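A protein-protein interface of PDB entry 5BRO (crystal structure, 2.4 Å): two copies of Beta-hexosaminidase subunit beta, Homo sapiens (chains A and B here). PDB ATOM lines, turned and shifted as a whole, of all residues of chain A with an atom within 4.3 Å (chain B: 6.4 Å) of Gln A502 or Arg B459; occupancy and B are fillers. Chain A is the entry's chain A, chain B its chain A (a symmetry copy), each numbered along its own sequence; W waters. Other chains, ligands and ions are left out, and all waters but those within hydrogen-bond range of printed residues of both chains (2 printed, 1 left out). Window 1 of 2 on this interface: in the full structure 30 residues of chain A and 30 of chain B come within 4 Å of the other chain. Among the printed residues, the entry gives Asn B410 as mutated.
The guanidinium group (NH2) of Arg A491 lies within salt-bridge range of the side-chain carboxylate (OD2) of Asp B452 (2.7 Å).
The backbone carbonyl oxygen (O) of Ala A501 is in hydrogen-bond range of the side-chain hydroxyl (OG1) of Thr B454, at 3.5 Å.
The side-chain amide oxygen of Gln A502 is in hydrogen-bond range of the side-chain amide nitrogen of Asn B455, at 2.9 Å.
NH2 of Arg B459 lies within hydrogen-bond range of OE1 of Gln A502, at 3.1 Å.
Water W1 lies within hydrogen-bond range of OE1 of Gln A502 (2.8 Å) and NH2 of Arg B459 (3.2 Å).
Water W2 lies within hydrogen-bond range of the guanidinium group (NH1) of Arg A491 (3.0 Å) and the side-chain carboxylate (OD2) of Asp B452 (3.4 Å).
6 positions are printed for both chains.
Of the 20 printed residues of chain B, 5 touch a printed residue of chain A.
Printed residues of chain B that touch a printed residue of chain A: Tyr B450, Asp B452, Thr B454, Asn B455 and Arg B459.
Hydrophobic or aromatic side chains of chain B within 4 Å of the printed part of chain A: Tyr B450.
Among the printed residues, 13 pairs touch across the chains.
Printed residues of chain B within 4 Å of Arg A491: Asp B452 (2.7 Å) and Thr B454 (3.8 Å).
Of the printed residues of chain A, Thr B454 touches Pro A458 (3.4 Å), Arg A491 (3.8 Å), Ala A500 (3.6 Å), Ala A501 (3.5 Å), Gln A502 (3.3 Å) and Pro A503 (3.9 Å).
Of the printed residues of chain A, Asn B455 touches Pro A458 and Gln A502.
The nearest printed residue of chain A that does not touch Arg B459 is Pro A458 (6.1 Å).
The nearest printed residue of chain A that does not touch Thr B454 is Trp A461 (6.7 Å).
Among the printed residues, pairs that only touch across the chains: Pro A458 with Thr B454 (3.4 Å), Pro A458 with Asn B455 (3.9 Å), Arg A491 with Thr B454 (3.8 Å), Ala A500 with Thr B454 (3.6 Å), Gln A502 with Thr B454 (3.3 Å), Pro A503 with Tyr B450 (3.6 Å), Pro A503 with Asp B452 (3.5 Å), Pro A503 with Thr B454 (3.9 Å) and Leu A504 with Tyr B450 (3.4 Å).
The side-chain amide nitrogen (NE2) of Gln A502 sits close to the backbone carbonyl oxygen (O) of Pro A458, at 3.3 Å.
The backbone carbonyl oxygen (O) of Trp A461 is in hydrogen-bond range of the backbone NH (N) of Gln A502.
The backbone carbonyl oxygen (O) of Ala A501 is in hydrogen-bond range of the guanidinium group (NE) of Arg A491 (2.9 Å).
The guanidinium group (NE) of Arg A491 sits at hydrogen-bond distance from the backbone carbonyl oxygen (O) of Gln A502 (3.3 Å).
The side-chain amide oxygen (OD1) of Asn B455 lies within hydrogen-bond range of the backbone NH (N) of Asp B452 (2.9 Å).
The guanidinium group of Arg B459 sits close to the side-chain amide nitrogen of Asn B455, at 3.4 Å.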
ATOM      1  N   PRO A 458       3.478  -8.786  -9.672  1.00  0.00           N
ATOM      2  CA  PRO A 458       3.989  -9.474 -10.862  1.00  0.00           C
ATOM      3  C   PRO A 458       5.080  -8.681 -11.612  1.00  0.00           C
ATOM      4  O   PRO A 458       5.900  -9.264 -12.295  1.00  0.00           O
ATOM      5  CB  PRO A 458       2.740  -9.669 -11.743  1.00  0.00           C
ATOM      6  CG  PRO A 458       1.683  -8.833 -11.140  1.00  0.00           C
ATOM      7  CD  PRO A 458       2.036  -8.552  -9.726  1.00  0.00           C
ATOM      8  N   TRP A 461       8.394  -9.795  -9.358  1.00  0.00           N
ATOM      9  CA  TRP A 461       8.821 -11.189  -9.268  1.00  0.00           C
ATOM     10  C   TRP A 461       8.297 -11.782 -10.487  1.00  0.00           C
ATOM     11  O   TRP A 461       7.108 -11.553 -10.787  1.00  0.00           O
ATOM     12  CB  TRP A 461       8.207 -11.893  -8.064  1.00  0.00           C
ATOM     13  CG  TRP A 461       8.374 -11.103  -6.814  1.00  0.00           C
ATOM     14  CD1 TRP A 461       7.441 -10.388  -6.197  1.00  0.00           C
ATOM     15  CD2 TRP A 461       9.558 -10.986  -6.038  1.00  0.00           C
ATOM     16  NE1 TRP A 461       7.965  -9.767  -5.089  1.00  0.00           N
ATOM     17  CE2 TRP A 461       9.291 -10.091  -5.008  1.00  0.00           C
ATOM     18  CE3 TRP A 461      10.853 -11.496  -6.168  1.00  0.00           C
ATOM     19  CZ2 TRP A 461      10.272  -9.661  -4.118  1.00  0.00           C
ATOM     20  CZ3 TRP A 461      11.816 -11.131  -5.238  1.00  0.00           C
ATOM     21  CH2 TRP A 461      11.524 -10.220  -4.226  1.00  0.00           C
ATOM     22  N   PRO A 462       9.125 -12.516 -11.233  1.00  0.00           N
ATOM     23  CA  PRO A 462      10.427 -13.004 -10.795  1.00  0.00           C
ATOM     24  C   PRO A 462      11.630 -12.198 -11.323  1.00  0.00           C
ATOM     25  O   PRO A 462      12.786 -12.590 -11.129  1.00  0.00           O
ATOM     26  CB  PRO A 462      10.503 -14.400 -11.414  1.00  0.00           C
ATOM     27  CG  PRO A 462       9.678 -14.261 -12.640  1.00  0.00           C
ATOM     28  CD  PRO A 462       8.512 -13.415 -12.231  1.00  0.00           C
ATOM     29  N   ARG A 463      11.366 -11.030 -11.867  1.00  0.00           N
ATOM     30  CA  ARG A 463      12.444 -10.261 -12.423  1.00  0.00           C
ATOM     31  C   ARG A 463      13.463  -9.981 -11.347  1.00  0.00           C
ATOM     32  O   ARG A 463      14.659 -10.049 -11.615  1.00  0.00           O
ATOM     33  CB  ARG A 463      11.943  -8.983 -13.110  1.00  0.00           C
ATOM     34  CG  ARG A 463      11.039  -9.268 -14.316  1.00  0.00           C
ATOM     35  CD  ARG A 463      10.883  -8.091 -15.292  1.00  0.00           C
ATOM     36  NE  ARG A 463      10.353  -6.975 -14.608  1.00  0.00           N
ATOM     37  CZ  ARG A 463      10.815  -5.745 -14.587  1.00  0.00           C
ATOM     38  NH1 ARG A 463      11.715  -5.288 -15.427  1.00  0.00           N
ATOM     39  NH2 ARG A 463      10.206  -4.920 -13.761  1.00  0.00           N
ATOM     40  N   ARG A 491       9.449 -19.795  -9.832  1.00  0.00           N
ATOM     41  CA  ARG A 491       8.339 -18.887 -10.052  1.00  0.00           C
ATOM     42  C   ARG A 491       7.039 -19.616  -9.879  1.00  0.00           C
ATOM     43  O   ARG A 491       6.167 -19.107  -9.230  1.00  0.00           O
ATOM     44  CB  ARG A 491       8.392 -18.251 -11.437  1.00  0.00           C
ATOM     45  CG  ARG A 491       7.162 -17.433 -11.829  1.00  0.00           C
ATOM     46  CD  ARG A 491       6.201 -18.251 -12.703  1.00  0.00           C
ATOM     47  NE  ARG A 491       4.938 -17.544 -12.888  1.00  0.00           N
ATOM     48  CZ  ARG A 491       3.941 -17.930 -13.677  1.00  0.00           C
ATOM     49  NH1 ARG A 491       4.018 -19.052 -14.367  1.00  0.00           N
ATOM     50  NH2 ARG A 491       2.849 -17.172 -13.783  1.00  0.00           N
ATOM     51  N   ALA A 500       1.794 -13.770  -6.650  1.00  0.00           N
ATOM     52  CA  ALA A 500       1.470 -13.701  -8.061  1.00  0.00           C
ATOM     53  C   ALA A 500       2.646 -13.237  -8.971  1.00  0.00           C
ATOM     54  O   ALA A 500       2.532 -12.258  -9.715  1.00  0.00           O
ATOM     55  CB  ALA A 500       0.259 -12.771  -8.244  1.00  0.00           C
ATOM     56  N   ALA A 501       3.707 -14.013  -9.019  1.00  0.00           N
ATOM     57  CA  ALA A 501       4.844 -13.705  -9.882  1.00  0.00           C
ATOM     58  C   ALA A 501       4.577 -14.077 -11.322  1.00  0.00           C
ATOM     59  O   ALA A 501       4.037 -15.138 -11.621  1.00  0.00           O
ATOM     60  CB  ALA A 501       6.092 -14.410  -9.384  1.00  0.00           C
ATOM     61  N   GLN A 502       4.988 -13.225 -12.241  1.00  0.00           N
ATOM     62  CA  GLN A 502       4.597 -13.462 -13.635  1.00  0.00           C
ATOM     63  C   GLN A 502       5.434 -14.478 -14.358  1.00  0.00           C
ATOM     64  O   GLN A 502       6.526 -14.837 -13.904  1.00  0.00           O
ATOM     65  CB  GLN A 502       4.604 -12.173 -14.422  1.00  0.00           C
ATOM     66  CG  GLN A 502       5.975 -11.601 -14.682  1.00  0.00           C
ATOM     67  CD  GLN A 502       5.896 -10.203 -15.256  1.00  0.00           C
ATOM     68  OE1 GLN A 502       4.824  -9.729 -15.653  1.00  0.00           O
ATOM     69  NE2 GLN A 502       7.029  -9.573 -15.375  1.00  0.00           N
ATOM     70  N   PRO A 503       4.927 -14.959 -15.501  1.00  0.00           N
ATOM     71  CA  PRO A 503       5.697 -15.919 -16.248  1.00  0.00           C
ATOM     72  C   PRO A 503       7.034 -15.385 -16.851  1.00  0.00           C
ATOM     73  O   PRO A 503       7.224 -14.171 -17.040  1.00  0.00           O
ATOM     74  CB  PRO A 503       4.752 -16.311 -17.358  1.00  0.00           C
ATOM     75  CG  PRO A 503       3.420 -15.740 -17.010  1.00  0.00           C
ATOM     76  CD  PRO A 503       3.727 -14.547 -16.247  1.00  0.00           C
ATOM     77  N   LEU A 504       7.956 -16.313 -17.110  1.00  0.00           N
ATOM     78  CA  LEU A 504       9.129 -16.025 -17.898  1.00  0.00           C
ATOM     79  C   LEU A 504       8.827 -16.131 -19.358  1.00  0.00           C
ATOM     80  O   LEU A 504       9.401 -15.389 -20.132  1.00  0.00           O
ATOM     81  CB  LEU A 504      10.265 -17.001 -17.604  1.00  0.00           C
ATOM     82  CG  LEU A 504      10.676 -17.192 -16.162  1.00  0.00           C
ATOM     83  CD1 LEU A 504      12.029 -17.836 -16.169  1.00  0.00           C
ATOM     84  CD2 LEU A 504      10.751 -15.891 -15.401  1.00  0.00           C
ATOM     85  N   LEU B 409      -0.644  -5.079 -27.306  1.00  0.00           N
ATOM     86  CA  LEU B 409      -0.468  -4.707 -25.921  1.00  0.00           C
ATOM     87  C   LEU B 409       0.384  -5.753 -25.171  1.00  0.00           C
ATOM     88  O   LEU B 409       0.869  -5.478 -24.096  1.00  0.00           O
ATOM     89  CB  LEU B 409      -1.830  -4.483 -25.238  1.00  0.00           C
ATOM     90  CG  LEU B 409      -2.413  -3.062 -25.263  1.00  0.00           C
ATOM     91  CD1 LEU B 409      -2.690  -2.590 -26.676  1.00  0.00           C
ATOM     92  CD2 LEU B 409      -3.716  -3.025 -24.477  1.00  0.00           C
ATOM     93  N   ASN B 410       0.671  -6.902 -25.766  1.00  0.00           N
ATOM     94  CA  ASN B 410       1.823  -7.727 -25.273  1.00  0.00           C
ATOM     95  C   ASN B 410       3.159  -7.017 -25.304  1.00  0.00           C
ATOM     96  O   ASN B 410       4.048  -7.331 -24.524  1.00  0.00           O
ATOM     97  CB  ASN B 410       1.952  -9.023 -26.054  1.00  0.00           C
ATOM     98  CG  ASN B 410       2.068  -8.781 -27.535  1.00  0.00           C
ATOM     99  OD1 ASN B 410       1.364  -7.950 -28.089  1.00  0.00           O
ATOM    100  ND2 ASN B 410       2.974  -9.477 -28.171  1.00  0.00           N
ATOM    101  N   ILE B 412       4.907  -4.422 -24.163  1.00  0.00           N
ATOM    102  CA  ILE B 412       4.947  -3.397 -23.121  1.00  0.00           C
ATOM    103  C   ILE B 412       6.132  -2.464 -23.280  1.00  0.00           C
ATOM    104  O   ILE B 412       7.084  -2.775 -23.951  1.00  0.00           O
ATOM    105  CB  ILE B 412       4.971  -4.077 -21.728  1.00  0.00           C
ATOM    106  CG1 ILE B 412       6.292  -4.810 -21.500  1.00  0.00           C
ATOM    107  CG2 ILE B 412       3.822  -5.093 -21.632  1.00  0.00           C
ATOM    108  CD1 ILE B 412       6.270  -5.773 -20.336  1.00  0.00           C
ATOM    109  N   LEU B 446      -3.552  -9.050 -26.734  1.00  0.00           N
ATOM    110  CA  LEU B 446      -2.644  -9.409 -25.631  1.00  0.00           C
ATOM    111  C   LEU B 446      -2.192 -10.869 -25.782  1.00  0.00           C
ATOM    112  O   LEU B 446      -2.672 -11.797 -25.112  1.00  0.00           O
ATOM    113  CB  LEU B 446      -3.275  -9.118 -24.264  1.00  0.00           C
ATOM    114  CG  LEU B 446      -2.382  -9.197 -23.029  1.00  0.00           C
ATOM    115  CD1 LEU B 446      -1.303  -8.117 -22.976  1.00  0.00           C
ATOM    116  CD2 LEU B 446      -3.229  -9.164 -21.760  1.00  0.00           C
ATOM    117  N   TYR B 450       4.123 -13.983 -22.552  1.00  0.00           N
ATOM    118  CA  TYR B 450       4.558 -13.395 -21.257  1.00  0.00           C
ATOM    119  C   TYR B 450       3.412 -13.131 -20.295  1.00  0.00           C
ATOM    120  O   TYR B 450       3.600 -12.511 -19.219  1.00  0.00           O
ATOM    121  CB  TYR B 450       5.405 -12.105 -21.453  1.00  0.00           C
ATOM    122  CG  TYR B 450       6.571 -12.356 -22.376  1.00  0.00           C
ATOM    123  CD1 TYR B 450       7.721 -12.968 -21.904  1.00  0.00           C
ATOM    124  CD2 TYR B 450       6.454 -12.169 -23.735  1.00  0.00           C
ATOM    125  CE1 TYR B 450       8.746 -13.333 -22.757  1.00  0.00           C
ATOM    126  CE2 TYR B 450       7.481 -12.515 -24.598  1.00  0.00           C
ATOM    127  CZ  TYR B 450       8.626 -13.094 -24.098  1.00  0.00           C
ATOM    128  OH  TYR B 450       9.660 -13.443 -24.903  1.00  0.00           O
ATOM    129  N   VAL B 451       2.243 -13.653 -20.636  1.00  0.00           N
ATOM    130  CA  VAL B 451       1.025 -13.346 -19.864  1.00  0.00           C
ATOM    131  C   VAL B 451       0.207 -14.529 -19.365  1.00  0.00           C
ATOM    132  O   VAL B 451      -0.207 -15.440 -20.143  1.00  0.00           O
ATOM    133  CB  VAL B 451       0.075 -12.451 -20.640  1.00  0.00           C
ATOM    134  CG1 VAL B 451      -1.171 -12.157 -19.803  1.00  0.00           C
ATOM    135  CG2 VAL B 451       0.778 -11.162 -21.032  1.00  0.00           C
ATOM    136  N   ASP B 452      -0.107 -14.469 -18.074  1.00  0.00           N
ATOM    137  CA  ASP B 452      -1.095 -15.395 -17.493  1.00  0.00           C
ATOM    138  C   ASP B 452      -1.935 -14.754 -16.375  1.00  0.00           C
ATOM    139  O   ASP B 452      -1.993 -13.498 -16.231  1.00  0.00           O
ATOM    140  CB  ASP B 452      -0.430 -16.727 -17.074  1.00  0.00           C
ATOM    141  CG  ASP B 452       0.254 -16.652 -15.735  1.00  0.00           C
ATOM    142  OD1 ASP B 452       0.406 -15.542 -15.160  1.00  0.00           O
ATOM    143  OD2 ASP B 452       0.688 -17.728 -15.254  1.00  0.00           O
ATOM    144  N   THR B 454      -1.606 -14.133 -13.522  1.00  0.00           N
ATOM    145  CA  THR B 454      -0.976 -13.330 -12.497  1.00  0.00           C
ATOM    146  C   THR B 454      -0.843 -11.897 -12.936  1.00  0.00           C
ATOM    147  O   THR B 454      -0.673 -11.031 -12.078  1.00  0.00           O
ATOM    148  CB  THR B 454       0.442 -13.837 -12.124  1.00  0.00           C
ATOM    149  OG1 THR B 454       1.287 -13.798 -13.278  1.00  0.00           O
ATOM    150  CG2 THR B 454       0.368 -15.245 -11.600  1.00  0.00           C
ATOM    151  N   ASN B 455      -0.792 -11.667 -14.250  1.00  0.00           N
ATOM    152  CA  ASN B 455      -0.431 -10.344 -14.759  1.00  0.00           C
ATOM    153  C   ASN B 455      -1.342  -9.784 -15.868  1.00  0.00           C
ATOM    154  O   ASN B 455      -1.341  -8.589 -16.109  1.00  0.00           O
ATOM    155  CB  ASN B 455       1.026 -10.317 -15.144  1.00  0.00           C
ATOM    156  CG  ASN B 455       1.326 -11.000 -16.469  1.00  0.00           C
ATOM    157  OD1 ASN B 455       0.619 -11.888 -16.914  1.00  0.00           O
ATOM    158  ND2 ASN B 455       2.446 -10.642 -17.054  1.00  0.00           N
ATOM    159  N   LEU B 456      -2.252 -10.613 -16.381  1.00  0.00           N
ATOM    160  CA  LEU B 456      -3.195 -10.232 -17.414  1.00  0.00           C
ATOM    161  C   LEU B 456      -3.882  -8.910 -17.153  1.00  0.00           C
ATOM    162  O   LEU B 456      -3.749  -7.971 -17.962  1.00  0.00           O
ATOM    163  CB  LEU B 456      -4.250 -11.326 -17.617  1.00  0.00           C
ATOM    164  CG  LEU B 456      -5.045 -11.246 -18.922  1.00  0.00           C
ATOM    165  CD1 LEU B 456      -5.340 -12.595 -19.519  1.00  0.00           C
ATOM    166  CD2 LEU B 456      -6.362 -10.535 -18.702  1.00  0.00           C
ATOM    167  N   THR B 457      -4.647  -8.847 -16.062  1.00  0.00           N
ATOM    168  CA  THR B 457      -5.541  -7.732 -15.816  1.00  0.00           C
ATOM    169  C   THR B 457      -4.839  -6.412 -15.690  1.00  0.00           C
ATOM    170  O   THR B 457      -5.232  -5.450 -16.326  1.00  0.00           O
ATOM    171  CB  THR B 457      -6.454  -8.018 -14.639  1.00  0.00           C
ATOM    172  OG1 THR B 457      -7.304  -9.113 -15.007  1.00  0.00           O
ATOM    173  CG2 THR B 457      -7.361  -6.877 -14.347  1.00  0.00           C
ATOM    174  N   PRO B 458      -3.728  -6.354 -14.964  1.00  0.00           N
ATOM    175  CA  PRO B 458      -3.150  -5.006 -14.952  1.00  0.00           C
ATOM    176  C   PRO B 458      -2.365  -4.660 -16.235  1.00  0.00           C
ATOM    177  O   PRO B 458      -2.235  -3.501 -16.580  1.00  0.00           O
ATOM    178  CB  PRO B 458      -2.227  -5.008 -13.719  1.00  0.00           C
ATOM    179  CG  PRO B 458      -2.117  -6.419 -13.296  1.00  0.00           C
ATOM    180  CD  PRO B 458      -3.263  -7.181 -13.851  1.00  0.00           C
ATOM    181  N   ARG B 459      -1.839  -5.647 -16.945  1.00  0.00           N
ATOM    182  CA  ARG B 459      -1.218  -5.333 -18.230  1.00  0.00           C
ATOM    183  C   ARG B 459      -2.274  -4.798 -19.228  1.00  0.00           C
ATOM    184  O   ARG B 459      -2.030  -3.846 -19.958  1.00  0.00           O
ATOM    185  CB  ARG B 459      -0.566  -6.567 -18.771  1.00  0.00           C
ATOM    186  CG  ARG B 459       0.194  -6.403 -20.062  1.00  0.00           C
ATOM    187  CD  ARG B 459       1.312  -7.433 -20.200  1.00  0.00           C
ATOM    188  NE  ARG B 459       2.286  -7.279 -19.115  1.00  0.00           N
ATOM    189  CZ  ARG B 459       3.386  -8.014 -18.991  1.00  0.00           C
ATOM    190  NH1 ARG B 459       3.688  -8.924 -19.919  1.00  0.00           N
ATOM    191  NH2 ARG B 459       4.187  -7.802 -17.948  1.00  0.00           N
ATOM    192  N   LEU B 460      -3.473  -5.362 -19.189  1.00  0.00           N
ATOM    193  CA  LEU B 460      -4.500  -5.075 -20.189  1.00  0.00           C
ATOM    194  C   LEU B 460      -5.200  -3.735 -19.920  1.00  0.00           C
ATOM    195  O   LEU B 460      -5.535  -3.025 -20.858  1.00  0.00           O
ATOM    196  CB  LEU B 460      -5.548  -6.189 -20.187  1.00  0.00           C
ATOM    197  CG  LEU B 460      -6.532  -6.126 -21.323  1.00  0.00           C
ATOM    198  CD1 LEU B 460      -5.773  -6.135 -22.646  1.00  0.00           C
ATOM    199  CD2 LEU B 460      -7.546  -7.255 -21.292  1.00  0.00           C
ATOM    200  N   TRP B 461      -5.524  -3.452 -18.658  1.00  0.00           N
ATOM    201  CA  TRP B 461      -6.357  -2.305 -18.308  1.00  0.00           C
ATOM    202  C   TRP B 461      -5.489  -1.503 -17.460  1.00  0.00           C
ATOM    203  O   TRP B 461      -4.871  -2.079 -16.542  1.00  0.00           O
ATOM    204  CB  TRP B 461      -7.588  -2.720 -17.512  1.00  0.00           C
ATOM    205  CG  TRP B 461      -8.313  -3.848 -18.159  1.00  0.00           C
ATOM    206  CD1 TRP B 461      -8.298  -5.120 -17.780  1.00  0.00           C
ATOM    207  CD2 TRP B 461      -9.170  -3.767 -19.289  1.00  0.00           C
ATOM    208  NE1 TRP B 461      -9.058  -5.884 -18.633  1.00  0.00           N
ATOM    209  CE2 TRP B 461      -9.564  -5.063 -19.603  1.00  0.00           C
ATOM    210  CE3 TRP B 461      -9.579  -2.719 -20.119  1.00  0.00           C
ATOM    211  CZ2 TRP B 461     -10.327  -5.361 -20.730  1.00  0.00           C
ATOM    212  CZ3 TRP B 461     -10.402  -3.000 -21.200  1.00  0.00           C
ATOM    213  CH2 TRP B 461     -10.768  -4.310 -21.500  1.00  0.00           C
ATOM    214  N   PRO B 462      -5.380  -0.201 -17.729  1.00  0.00           N
ATOM    215  CA  PRO B 462      -6.264   0.541 -18.621  1.00  0.00           C
ATOM    216  C   PRO B 462      -5.684   0.816 -20.023  1.00  0.00           C
ATOM    217  O   PRO B 462      -6.283   1.545 -20.820  1.00  0.00           O
ATOM    218  CB  PRO B 462      -6.418   1.889 -17.916  1.00  0.00           C
ATOM    219  CG  PRO B 462      -5.131   2.031 -17.191  1.00  0.00           C
ATOM    220  CD  PRO B 462      -4.828   0.661 -16.666  1.00  0.00           C
ATOM    221  N   ARG B 463      -4.607   0.141 -20.360  1.00  0.00           N
ATOM    222  CA  ARG B 463      -3.995   0.397 -21.633  1.00  0.00           C
ATOM    223  C   ARG B 463      -4.995   0.128 -22.729  1.00  0.00           C
ATOM    224  O   ARG B 463      -5.054   0.886 -23.693  1.00  0.00           O
ATOM    225  CB  ARG B 463      -2.693  -0.395 -21.814  1.00  0.00           C
ATOM    226  CG  ARG B 463      -1.609   0.000 -20.804  1.00  0.00           C
ATOM    227  CD  ARG B 463      -0.181  -0.406 -21.205  1.00  0.00           C
ATOM    228  NE  ARG B 463      -0.119  -1.806 -21.382  1.00  0.00           N
ATOM    229  CZ  ARG B 463       0.353  -2.470 -22.414  1.00  0.00           C
ATOM    230  NH1 ARG B 463       1.095  -1.930 -23.353  1.00  0.00           N
ATOM    231  NH2 ARG B 463       0.171  -3.774 -22.385  1.00  0.00           N
ATOM    232  N   ALA B 464      -5.827  -0.889 -22.578  1.00  0.00           N
ATOM    233  CA  ALA B 464      -6.784  -1.208 -23.624  1.00  0.00           C
ATOM    234  C   ALA B 464      -7.964  -0.250 -23.634  1.00  0.00           C
ATOM    235  O   ALA B 464      -8.734  -0.246 -24.594  1.00  0.00           O
ATOM    236  CB  ALA B 464      -7.324  -2.616 -23.456  1.00  0.00           C
ATOM    237  N   ALA B 500      -8.325  -5.180 -11.183  1.00  0.00           N
ATOM    238  CA  ALA B 500      -7.021  -4.653 -10.834  1.00  0.00           C
ATOM    239  C   ALA B 500      -6.274  -3.952 -12.007  1.00  0.00           C
ATOM    240  O   ALA B 500      -5.148  -4.317 -12.358  1.00  0.00           O
ATOM    241  CB  ALA B 500      -6.163  -5.798 -10.268  1.00  0.00           C
ATOM    242  N   GLN B 502      -3.978  -1.151 -13.759  1.00  0.00           N
ATOM    243  CA  GLN B 502      -2.820  -0.449 -13.196  1.00  0.00           C
ATOM    244  C   GLN B 502      -2.867   1.047 -13.329  1.00  0.00           C
ATOM    245  O   GLN B 502      -3.658   1.588 -14.109  1.00  0.00           O
ATOM    246  CB  GLN B 502      -1.535  -0.954 -13.808  1.00  0.00           C
ATOM    247  CG  GLN B 502      -1.332  -0.572 -15.253  1.00  0.00           C
ATOM    248  CD  GLN B 502      -0.159  -1.305 -15.864  1.00  0.00           C
ATOM    249  OE1 GLN B 502       0.634  -1.949 -15.165  1.00  0.00           O
ATOM    250  NE2 GLN B 502       0.003  -1.151 -17.147  1.00  0.00           N
HETATM  251  O   HOH W   1       3.784  -7.298 -14.840  1.00  0.00           O
HETATM  252  O   HOH W   2       2.129 -20.665 -16.032  1.00  0.00           O
